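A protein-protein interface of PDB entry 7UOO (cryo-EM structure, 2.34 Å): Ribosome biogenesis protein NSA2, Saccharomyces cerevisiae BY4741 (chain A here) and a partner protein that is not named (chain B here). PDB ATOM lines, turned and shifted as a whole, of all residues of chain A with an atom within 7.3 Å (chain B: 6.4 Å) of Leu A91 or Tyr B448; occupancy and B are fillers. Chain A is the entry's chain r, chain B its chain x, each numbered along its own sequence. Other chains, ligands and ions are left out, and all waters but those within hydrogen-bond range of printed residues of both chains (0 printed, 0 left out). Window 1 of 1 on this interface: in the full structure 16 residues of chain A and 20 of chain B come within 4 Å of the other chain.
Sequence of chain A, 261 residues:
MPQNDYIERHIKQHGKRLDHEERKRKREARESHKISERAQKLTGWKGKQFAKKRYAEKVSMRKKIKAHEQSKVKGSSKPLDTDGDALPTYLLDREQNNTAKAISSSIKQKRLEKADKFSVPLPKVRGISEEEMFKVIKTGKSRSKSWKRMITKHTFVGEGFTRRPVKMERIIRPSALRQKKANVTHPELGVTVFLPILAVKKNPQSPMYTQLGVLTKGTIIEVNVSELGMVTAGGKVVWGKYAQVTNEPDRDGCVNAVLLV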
ATOM      1  N   LEU A  87      18.964  16.849   2.427  1.00  0.00           N
ATOM      2  CA  LEU A  87      18.828  17.117   1.004  1.00  0.00           C
ATOM      3  C   LEU A  87      17.919  16.082   0.345  1.00  0.00           C
ATOM      4  O   LEU A  87      17.804  14.952   0.828  1.00  0.00           O
ATOM      5  CB  LEU A  87      20.198  17.100   0.330  1.00  0.00           C
ATOM      6  CG  LEU A  87      21.161  18.224   0.719  1.00  0.00           C
ATOM      7  CD1 LEU A  87      22.549  17.962   0.164  1.00  0.00           C
ATOM      8  CD2 LEU A  87      20.634  19.566   0.236  1.00  0.00           C
ATOM      9  N   PRO A  88      17.251  16.439  -0.764  1.00  0.00           N
ATOM     10  CA  PRO A  88      16.441  15.447  -1.488  1.00  0.00           C
ATOM     11  C   PRO A  88      17.294  14.436  -2.237  1.00  0.00           C
ATOM     12  O   PRO A  88      18.525  14.519  -2.214  1.00  0.00           O
ATOM     13  CB  PRO A  88      15.611  16.303  -2.457  1.00  0.00           C
ATOM     14  CG  PRO A  88      15.726  17.700  -1.953  1.00  0.00           C
ATOM     15  CD  PRO A  88      17.057  17.797  -1.295  1.00  0.00           C
ATOM     16  N   THR A  89      16.646  13.478  -2.906  1.00  0.00           N
ATOM     17  CA  THR A  89      17.380  12.426  -3.607  1.00  0.00           C
ATOM     18  C   THR A  89      18.193  12.985  -4.769  1.00  0.00           C
ATOM     19  O   THR A  89      19.339  12.575  -4.983  1.00  0.00           O
ATOM     20  CB  THR A  89      16.417  11.350  -4.110  1.00  0.00           C
ATOM     21  OG1 THR A  89      15.524  11.919  -5.076  1.00  0.00           O
ATOM     22  CG2 THR A  89      15.612  10.772  -2.957  1.00  0.00           C
ATOM     23  N   TYR A  90      17.621  13.915  -5.531  1.00  0.00           N
ATOM     24  CA  TYR A  90      18.317  14.457  -6.690  1.00  0.00           C
ATOM     25  C   TYR A  90      19.387  15.477  -6.319  1.00  0.00           C
ATOM     26  O   TYR A  90      20.144  15.899  -7.199  1.00  0.00           O
ATOM     27  CB  TYR A  90      17.312  15.082  -7.664  1.00  0.00           C
ATOM     28  CG  TYR A  90      16.419  16.139  -7.054  1.00  0.00           C
ATOM     29  CD1 TYR A  90      16.800  17.473  -7.038  1.00  0.00           C
ATOM     30  CD2 TYR A  90      15.190  15.802  -6.500  1.00  0.00           C
ATOM     31  CE1 TYR A  90      15.988  18.441  -6.483  1.00  0.00           C
ATOM     32  CE2 TYR A  90      14.371  16.764  -5.944  1.00  0.00           C
ATOM     33  CZ  TYR A  90      14.776  18.082  -5.939  1.00  0.00           C
ATOM     34  OH  TYR A  90      13.967  19.045  -5.387  1.00  0.00           O
ATOM     35  N   LEU A  91      19.475  15.882  -5.051  1.00  0.00           N
ATOM     36  CA  LEU A  91      20.497  16.823  -4.622  1.00  0.00           C
ATOM     37  C   LEU A  91      21.626  16.191  -3.825  1.00  0.00           C
ATOM     38  O   LEU A  91      22.703  16.787  -3.742  1.00  0.00           O
ATOM     39  CB  LEU A  91      19.875  17.959  -3.794  1.00  0.00           C
ATOM     40  CG  LEU A  91      19.031  18.957  -4.592  1.00  0.00           C
ATOM     41  CD1 LEU A  91      18.735  20.200  -3.771  1.00  0.00           C
ATOM     42  CD2 LEU A  91      19.711  19.324  -5.903  1.00  0.00           C
ATOM     43  N   LEU A  92      21.420  15.014  -3.242  1.00  0.00           N
ATOM     44  CA  LEU A  92      22.542  14.317  -2.639  1.00  0.00           C
ATOM     45  C   LEU A  92      23.454  13.768  -3.735  1.00  0.00           C
ATOM     46  O   LEU A  92      23.090  13.713  -4.914  1.00  0.00           O
ATOM     47  CB  LEU A  92      22.058  13.213  -1.695  1.00  0.00           C
ATOM     48  CG  LEU A  92      20.930  12.267  -2.104  1.00  0.00           C
ATOM     49  CD1 LEU A  92      21.444  11.090  -2.925  1.00  0.00           C
ATOM     50  CD2 LEU A  92      20.186  11.781  -0.869  1.00  0.00           C
ATOM     51  N   ASP A  93      24.665  13.378  -3.325  1.00  0.00           N
ATOM     52  CA  ASP A  93      25.789  13.068  -4.212  1.00  0.00           C
ATOM     53  C   ASP A  93      26.220  14.277  -5.037  1.00  0.00           C
ATOM     54  O   ASP A  93      26.833  14.125  -6.097  1.00  0.00           O
ATOM     55  CB  ASP A  93      25.493  11.877  -5.134  1.00  0.00           C
ATOM     56  CG  ASP A  93      25.180  10.611  -4.367  1.00  0.00           C
ATOM     57  OD1 ASP A  93      25.857  10.348  -3.352  1.00  0.00           O
ATOM     58  OD2 ASP A  93      24.253   9.885  -4.780  1.00  0.00           O
ATOM     59  N   ARG A  94      25.907  15.480  -4.559  1.00  0.00           N
ATOM     60  CA  ARG A  94      26.337  16.725  -5.176  1.00  0.00           C
ATOM     61  C   ARG A  94      26.920  17.632  -4.103  1.00  0.00           C
ATOM     62  O   ARG A  94      26.524  17.569  -2.937  1.00  0.00           O
ATOM     63  CB  ARG A  94      25.180  17.444  -5.886  1.00  0.00           C
ATOM     64  CG  ARG A  94      24.482  16.626  -6.958  1.00  0.00           C
ATOM     65  CD  ARG A  94      23.534  17.493  -7.770  1.00  0.00           C
ATOM     66  NE  ARG A  94      22.802  16.724  -8.769  1.00  0.00           N
ATOM     67  CZ  ARG A  94      23.265  16.435  -9.976  1.00  0.00           C
ATOM     68  NH1 ARG A  94      24.462  16.833 -10.371  1.00  0.00           N
ATOM     69  NH2 ARG A  94      22.511  15.722 -10.806  1.00  0.00           N
ATOM     70  N   GLU A  95      27.864  18.475  -4.505  1.00  0.00           N
ATOM     71  CA  GLU A  95      28.507  19.423  -3.606  1.00  0.00           C
ATOM     72  C   GLU A  95      28.107  20.849  -3.972  1.00  0.00           C
ATOM     73  O   GLU A  95      27.274  21.084  -4.852  1.00  0.00           O
ATOM     74  CB  GLU A  95      30.028  19.253  -3.636  1.00  0.00           C
ATOM     75  CG  GLU A  95      30.526  18.007  -2.918  1.00  0.00           C
ATOM     76  CD  GLU A  95      31.976  18.124  -2.480  1.00  0.00           C
ATOM     77  OE1 GLU A  95      32.730  18.899  -3.105  1.00  0.00           O
ATOM     78  OE2 GLU A  95      32.357  17.446  -1.503  1.00  0.00           O
ATOM     79  N   ASN B 406      17.443  18.371 -14.734  1.00  0.00           N
ATOM     80  CA  ASN B 406      17.140  17.708 -13.475  1.00  0.00           C
ATOM     81  C   ASN B 406      15.843  16.915 -13.528  1.00  0.00           C
ATOM     82  O   ASN B 406      15.755  15.839 -12.928  1.00  0.00           O
ATOM     83  CB  ASN B 406      17.073  18.733 -12.340  1.00  0.00           C
ATOM     84  CG  ASN B 406      16.855  18.089 -10.987  1.00  0.00           C
ATOM     85  OD1 ASN B 406      17.769  17.500 -10.413  1.00  0.00           O
ATOM     86  ND2 ASN B 406      15.641  18.204 -10.465  1.00  0.00           N
ATOM     87  N   HIS B 407      14.827  17.410 -14.230  1.00  0.00           N
ATOM     88  CA  HIS B 407      13.542  16.729 -14.242  1.00  0.00           C
ATOM     89  C   HIS B 407      12.996  16.659 -15.659  1.00  0.00           C
ATOM     90  O   HIS B 407      13.252  17.536 -16.483  1.00  0.00           O
ATOM     91  CB  HIS B 407      12.534  17.431 -13.325  1.00  0.00           C
ATOM     92  CG  HIS B 407      11.471  16.524 -12.792  1.00  0.00           C
ATOM     93  ND1 HIS B 407      10.202  16.468 -13.325  1.00  0.00           N
ATOM     94  CD2 HIS B 407      11.487  15.640 -11.767  1.00  0.00           C
ATOM     95  CE1 HIS B 407       9.482  15.587 -12.653  1.00  0.00           C
ATOM     96  NE2 HIS B 407      10.240  15.070 -11.704  1.00  0.00           N
ATOM     97  N   ALA B 420      12.883  20.342 -17.007  1.00  0.00           N
ATOM     98  CA  ALA B 420      13.280  21.396 -16.083  1.00  0.00           C
ATOM     99  C   ALA B 420      14.767  21.249 -15.798  1.00  0.00           C
ATOM    100  O   ALA B 420      15.208  20.182 -15.344  1.00  0.00           O
ATOM    101  CB  ALA B 420      12.474  21.320 -14.788  1.00  0.00           C
ATOM    102  N   SER B 421      15.532  22.315 -16.052  1.00  0.00           N
ATOM    103  CA  SER B 421      16.983  22.238 -15.966  1.00  0.00           C
ATOM    104  C   SER B 421      17.523  23.154 -14.874  1.00  0.00           C
ATOM    105  O   SER B 421      16.798  23.952 -14.277  1.00  0.00           O
ATOM    106  CB  SER B 421      17.623  22.590 -17.312  1.00  0.00           C
ATOM    107  OG  SER B 421      18.991  22.920 -17.163  1.00  0.00           O
ATOM    108  N   PHE B 422      18.827  23.028 -14.627  1.00  0.00           N
ATOM    109  CA  PHE B 422      19.521  23.860 -13.652  1.00  0.00           C
ATOM    110  C   PHE B 422      19.939  25.212 -14.212  1.00  0.00           C
ATOM    111  O   PHE B 422      20.501  26.021 -13.467  1.00  0.00           O
ATOM    112  CB  PHE B 422      20.756  23.136 -13.109  1.00  0.00           C
ATOM    113  CG  PHE B 422      20.477  22.272 -11.914  1.00  0.00           C
ATOM    114  CD1 PHE B 422      19.184  21.898 -11.593  1.00  0.00           C
ATOM    115  CD2 PHE B 422      21.512  21.847 -11.101  1.00  0.00           C
ATOM    116  CE1 PHE B 422      18.930  21.108 -10.493  1.00  0.00           C
ATOM    117  CE2 PHE B 422      21.262  21.056  -9.998  1.00  0.00           C
ATOM    118  CZ  PHE B 422      19.969  20.686  -9.696  1.00  0.00           C
ATOM    119  N   SER B 446      17.743  27.659 -10.200  1.00  0.00           N
ATOM    120  CA  SER B 446      17.579  26.373 -10.864  1.00  0.00           C
ATOM    121  C   SER B 446      16.227  25.749 -10.539  1.00  0.00           C
ATOM    122  O   SER B 446      15.772  25.772  -9.393  1.00  0.00           O
ATOM    123  CB  SER B 446      18.707  25.424 -10.457  1.00  0.00           C
ATOM    124  OG  SER B 446      18.654  25.123  -9.077  1.00  0.00           O
ATOM    125  N   VAL B 447      15.586  25.190 -11.562  1.00  0.00           N
ATOM    126  CA  VAL B 447      14.283  24.552 -11.417  1.00  0.00           C
ATOM    127  C   VAL B 447      14.490  23.116 -10.963  1.00  0.00           C
ATOM    128  O   VAL B 447      15.210  22.347 -11.610  1.00  0.00           O
ATOM    129  CB  VAL B 447      13.494  24.600 -12.735  1.00  0.00           C
ATOM    130  CG1 VAL B 447      12.058  24.155 -12.503  1.00  0.00           C
ATOM    131  CG2 VAL B 447      13.543  25.991 -13.337  1.00  0.00           C
ATOM    132  N   TYR B 448      13.851  22.748  -9.857  1.00  0.00           N
ATOM    133  CA  TYR B 448      14.051  21.421  -9.292  1.00  0.00           C
ATOM    134  C   TYR B 448      13.108  20.384  -9.893  1.00  0.00           C
ATOM    135  O   TYR B 448      13.567  19.359 -10.404  1.00  0.00           O
ATOM    136  CB  TYR B 448      13.909  21.475  -7.771  1.00  0.00           C
ATOM    137  CG  TYR B 448      15.117  22.082  -7.100  1.00  0.00           C
ATOM    138  CD1 TYR B 448      16.387  21.899  -7.627  1.00  0.00           C
ATOM    139  CD2 TYR B 448      14.988  22.851  -5.953  1.00  0.00           C
ATOM    140  CE1 TYR B 448      17.496  22.451  -7.026  1.00  0.00           C
ATOM    141  CE2 TYR B 448      16.093  23.410  -5.345  1.00  0.00           C
ATOM    142  CZ  TYR B 448      17.344  23.207  -5.886  1.00  0.00           C
ATOM    143  OH  TYR B 448      18.449  23.760  -5.284  1.00  0.00           O
ATOM    144  N   GLN B 449      11.798  20.624  -9.855  1.00  0.00           N
ATOM    145  CA  GLN B 449      10.878  19.654 -10.430  1.00  0.00           C
ATOM    146  C   GLN B 449       9.602  20.340 -10.903  1.00  0.00           C
ATOM    147  O   GLN B 449       9.354  21.527 -10.643  1.00  0.00           O
ATOM    148  CB  GLN B 449      10.567  18.516  -9.445  1.00  0.00           C
ATOM    149  CG  GLN B 449       9.519  18.817  -8.400  1.00  0.00           C
ATOM    150  CD  GLN B 449       9.252  17.625  -7.501  1.00  0.00           C
ATOM    151  OE1 GLN B 449       8.238  17.572  -6.806  1.00  0.00           O
ATOM    152  NE2 GLN B 449      10.164  16.660  -7.510  1.00  0.00           N
ATOM    153  N   VAL B 450       8.798  19.551 -11.621  1.00  0.00           N
ATOM    154  CA  VAL B 450       7.685  20.032 -12.428  1.00  0.00           C
ATOM    155  C   VAL B 450       6.537  19.033 -12.317  1.00  0.00           C
ATOM    156  O   VAL B 450       6.721  17.880 -11.922  1.00  0.00           O
ATOM    157  CB  VAL B 450       8.123  20.225 -13.901  1.00  0.00           C
ATOM    158  CG1 VAL B 450       8.003  18.925 -14.687  1.00  0.00           C
ATOM    159  CG2 VAL B 450       7.357  21.345 -14.553  1.00  0.00           C
ATOM    160  N   CYS B 462       8.521  24.154  -9.433  1.00  0.00           N
ATOM    161  CA  CYS B 462       9.088  24.703  -8.208  1.00  0.00           C
ATOM    162  C   CYS B 462      10.562  24.999  -8.435  1.00  0.00           C
ATOM    163  O   CYS B 462      11.236  24.274  -9.174  1.00  0.00           O
ATOM    164  CB  CYS B 462       8.920  23.735  -7.035  1.00  0.00           C
ATOM    165  SG  CYS B 462       9.803  22.175  -7.218  1.00  0.00           S
ATOM    166  N   SER B 463      11.073  26.065  -7.820  1.00  0.00           N
ATOM    167  CA  SER B 463      12.458  26.423  -8.092  1.00  0.00           C
ATOM    168  C   SER B 463      13.236  26.707  -6.814  1.00  0.00           C
ATOM    169  O   SER B 463      12.684  26.790  -5.714  1.00  0.00           O
ATOM    170  CB  SER B 463      12.542  27.628  -9.033  1.00  0.00           C
ATOM    171  OG  SER B 463      13.886  27.975  -9.305  1.00  0.00           O
ATOM    172  N   LYS B 464      14.552  26.844  -6.995  1.00  0.00           N
ATOM    173  CA  LYS B 464      15.468  27.200  -5.920  1.00  0.00           C
ATOM    174  C   LYS B 464      15.289  28.645  -5.465  1.00  0.00           C
ATOM    175  O   LYS B 464      15.742  28.998  -4.372  1.00  0.00           O
ATOM    176  CB  LYS B 464      16.906  26.948  -6.393  1.00  0.00           C
ATOM    177  CG  LYS B 464      18.005  27.099  -5.355  1.00  0.00           C
ATOM    178  CD  LYS B 464      19.369  26.894  -5.996  1.00  0.00           C
ATOM    179  CE  LYS B 464      20.492  26.953  -4.977  1.00  0.00           C
ATOM    180  NZ  LYS B 464      20.718  28.329  -4.465  1.00  0.00           N
ATOM    181  N   ASP B 465      14.610  29.478  -6.256  1.00  0.00           N
ATOM    182  CA  ASP B 465      14.391  30.878  -5.916  1.00  0.00           C
ATOM    183  C   ASP B 465      13.157  31.085  -5.041  1.00  0.00           C
ATOM    184  O   ASP B 465      12.590  32.185  -5.040  1.00  0.00           O
ATOM    185  CB  ASP B 465      14.296  31.732  -7.186  1.00  0.00           C
ATOM    186  CG  ASP B 465      13.069  31.421  -8.036  1.00  0.00           C
ATOM    187  OD1 ASP B 465      12.328  30.463  -7.738  1.00  0.00           O
ATOM    188  OD2 ASP B 465      12.839  32.155  -9.018  1.00  0.00           O
ATOM    189  N   GLU B 488      14.134  27.402  -0.018  1.00  0.00           N
ATOM    190  CA  GLU B 488      14.084  26.613  -1.244  1.00  0.00           C
ATOM    191  C   GLU B 488      12.937  25.613  -1.215  1.00  0.00           C
ATOM    192  O   GLU B 488      12.659  24.989  -0.189  1.00  0.00           O
ATOM    193  CB  GLU B 488      15.406  25.872  -1.452  1.00  0.00           C
ATOM    194  CG  GLU B 488      16.626  26.768  -1.568  1.00  0.00           C
ATOM    195  CD  GLU B 488      17.886  25.989  -1.894  1.00  0.00           C
ATOM    196  OE1 GLU B 488      17.788  24.762  -2.106  1.00  0.00           O
ATOM    197  OE2 GLU B 488      18.973  26.601  -1.939  1.00  0.00           O
ATOM    198  N   VAL B 489      12.266  25.470  -2.355  1.00  0.00           N
ATOM    199  CA  VAL B 489      11.177  24.516  -2.525  1.00  0.00           C
ATOM    200  C   VAL B 489      11.740  23.267  -3.186  1.00  0.00           C
ATOM    201  O   VAL B 489      12.397  23.350  -4.231  1.00  0.00           O
ATOM    202  CB  VAL B 489      10.036  25.113  -3.366  1.00  0.00           C
ATOM    203  CG1 VAL B 489       8.819  24.205  -3.325  1.00  0.00           C
ATOM    204  CG2 VAL B 489       9.696  26.509  -2.884  1.00  0.00           C
ATOM    205  N   TYR B 490      11.481  22.108  -2.586  1.00  0.00           N
ATOM    206  CA  TYR B 490      12.020  20.850  -3.079  1.00  0.00           C
ATOM    207  C   TYR B 490      10.996  19.963  -3.761  1.00  0.00           C
ATOM    208  O   TYR B 490      11.360  19.216  -4.671  1.00  0.00           O
ATOM    209  CB  TYR B 490      12.660  20.060  -1.934  1.00  0.00           C
ATOM    210  CG  TYR B 490      13.961  20.642  -1.444  1.00  0.00           C
ATOM    211  CD1 TYR B 490      14.865  21.215  -2.328  1.00  0.00           C
ATOM    212  CD2 TYR B 490      14.285  20.620  -0.097  1.00  0.00           C
ATOM    213  CE1 TYR B 490      16.053  21.750  -1.883  1.00  0.00           C
ATOM    214  CE2 TYR B 490      15.470  21.147   0.356  1.00  0.00           C
ATOM    215  CZ  TYR B 490      16.351  21.713  -0.538  1.00  0.00           C
ATOM    216  OH  TYR B 490      17.534  22.242  -0.083  1.00  0.00           O
ATOM    217  N   THR B 491       9.733  20.013  -3.350  1.00  0.00           N
ATOM    218  CA  THR B 491       8.724  19.125  -3.905  1.00  0.00           C
ATOM    219  C   THR B 491       7.460  19.903  -4.240  1.00  0.00           C
ATOM    220  O   THR B 491       7.072  20.825  -3.514  1.00  0.00           O
ATOM    221  CB  THR B 491       8.407  17.972  -2.934  1.00  0.00           C
ATOM    222  OG1 THR B 491       7.316  17.195  -3.442  1.00  0.00           O
ATOM    223  CG2 THR B 491       8.060  18.505  -1.554  1.00  0.00           C
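The side-chain hydroxyl (OH) of Tyr A90 lies within hydrogen-bond range of the backbone carbonyl oxygen (O) of Tyr B490, 2.7 Å away.
The side-chain hydroxyl of Tyr B448 lies within hydrogen-bond range of the side-chain carboxylate of Glu B488, 3.4 Å away.
OE1 of Glu B488 is in hydrogen-bond range of OH of Tyr B490 (3.2 Å).
O of Tyr A90 sits at hydrogen-bond distance from NE of Arg A94 (3.2 Å).
The backbone NH (N) of Tyr B448 sits at hydrogen-bond distance from the backbone carbonyl oxygen (O) of Cys B462 (3.1 Å).
N of Asn B406 sits at hydrogen-bond distance from O of Ala B420 (2.9 Å).
Tyr B490 touches Pro A88 (CG to CG, 3.5 Å).
OD1 of Asn B406 touches CD1 of Tyr A90, 3.5 Å away.
Tyr A90 touches Tyr B448.
CD1 of Leu A91 touches OH of Tyr B448, at 3.9 Å.
Tyr B490 touches Leu A91 (CE1 to CD1, 3.6 Å).
Of chain B, only Tyr B448 (3.9 Å) and Tyr B490 (3.6 Å) come within 4 Å of Leu A91.
Of chain A, only Tyr A90 and Leu A91 come within 4 Å of Tyr B448.
Of the printed residues of chain B, Pro A88 touches Tyr B490.
Of the printed residues of chain B, Tyr A90 touches Asn B406, Tyr B448 and Tyr B490.
Of the printed residues of chain A, Tyr B490 touches Pro A88, Tyr A90 and Leu A91.
Of the printed residues of chain A, Asn B406 touches Tyr A90.
Printed residues of chain A that touch a printed residue of chain B: Pro A88, Tyr A90 and Leu A91.
Hydrophobic or aromatic side chains of chain A that line the printed part of chain B: Pro A88, Tyr A90 and Leu A91.
Along chain A the printed residues that touch a printed residue of chain B span positions 88 to 91.
Of the 18 printed residues of chain B, 3 touch a printed residue of chain A.
Among the printed residues, 6 pairs touch across the chains.
Among the printed residues, no Asp or Glu carboxylate lies within 4 Å of a Lys or Arg side-chain nitrogen of the other chain.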
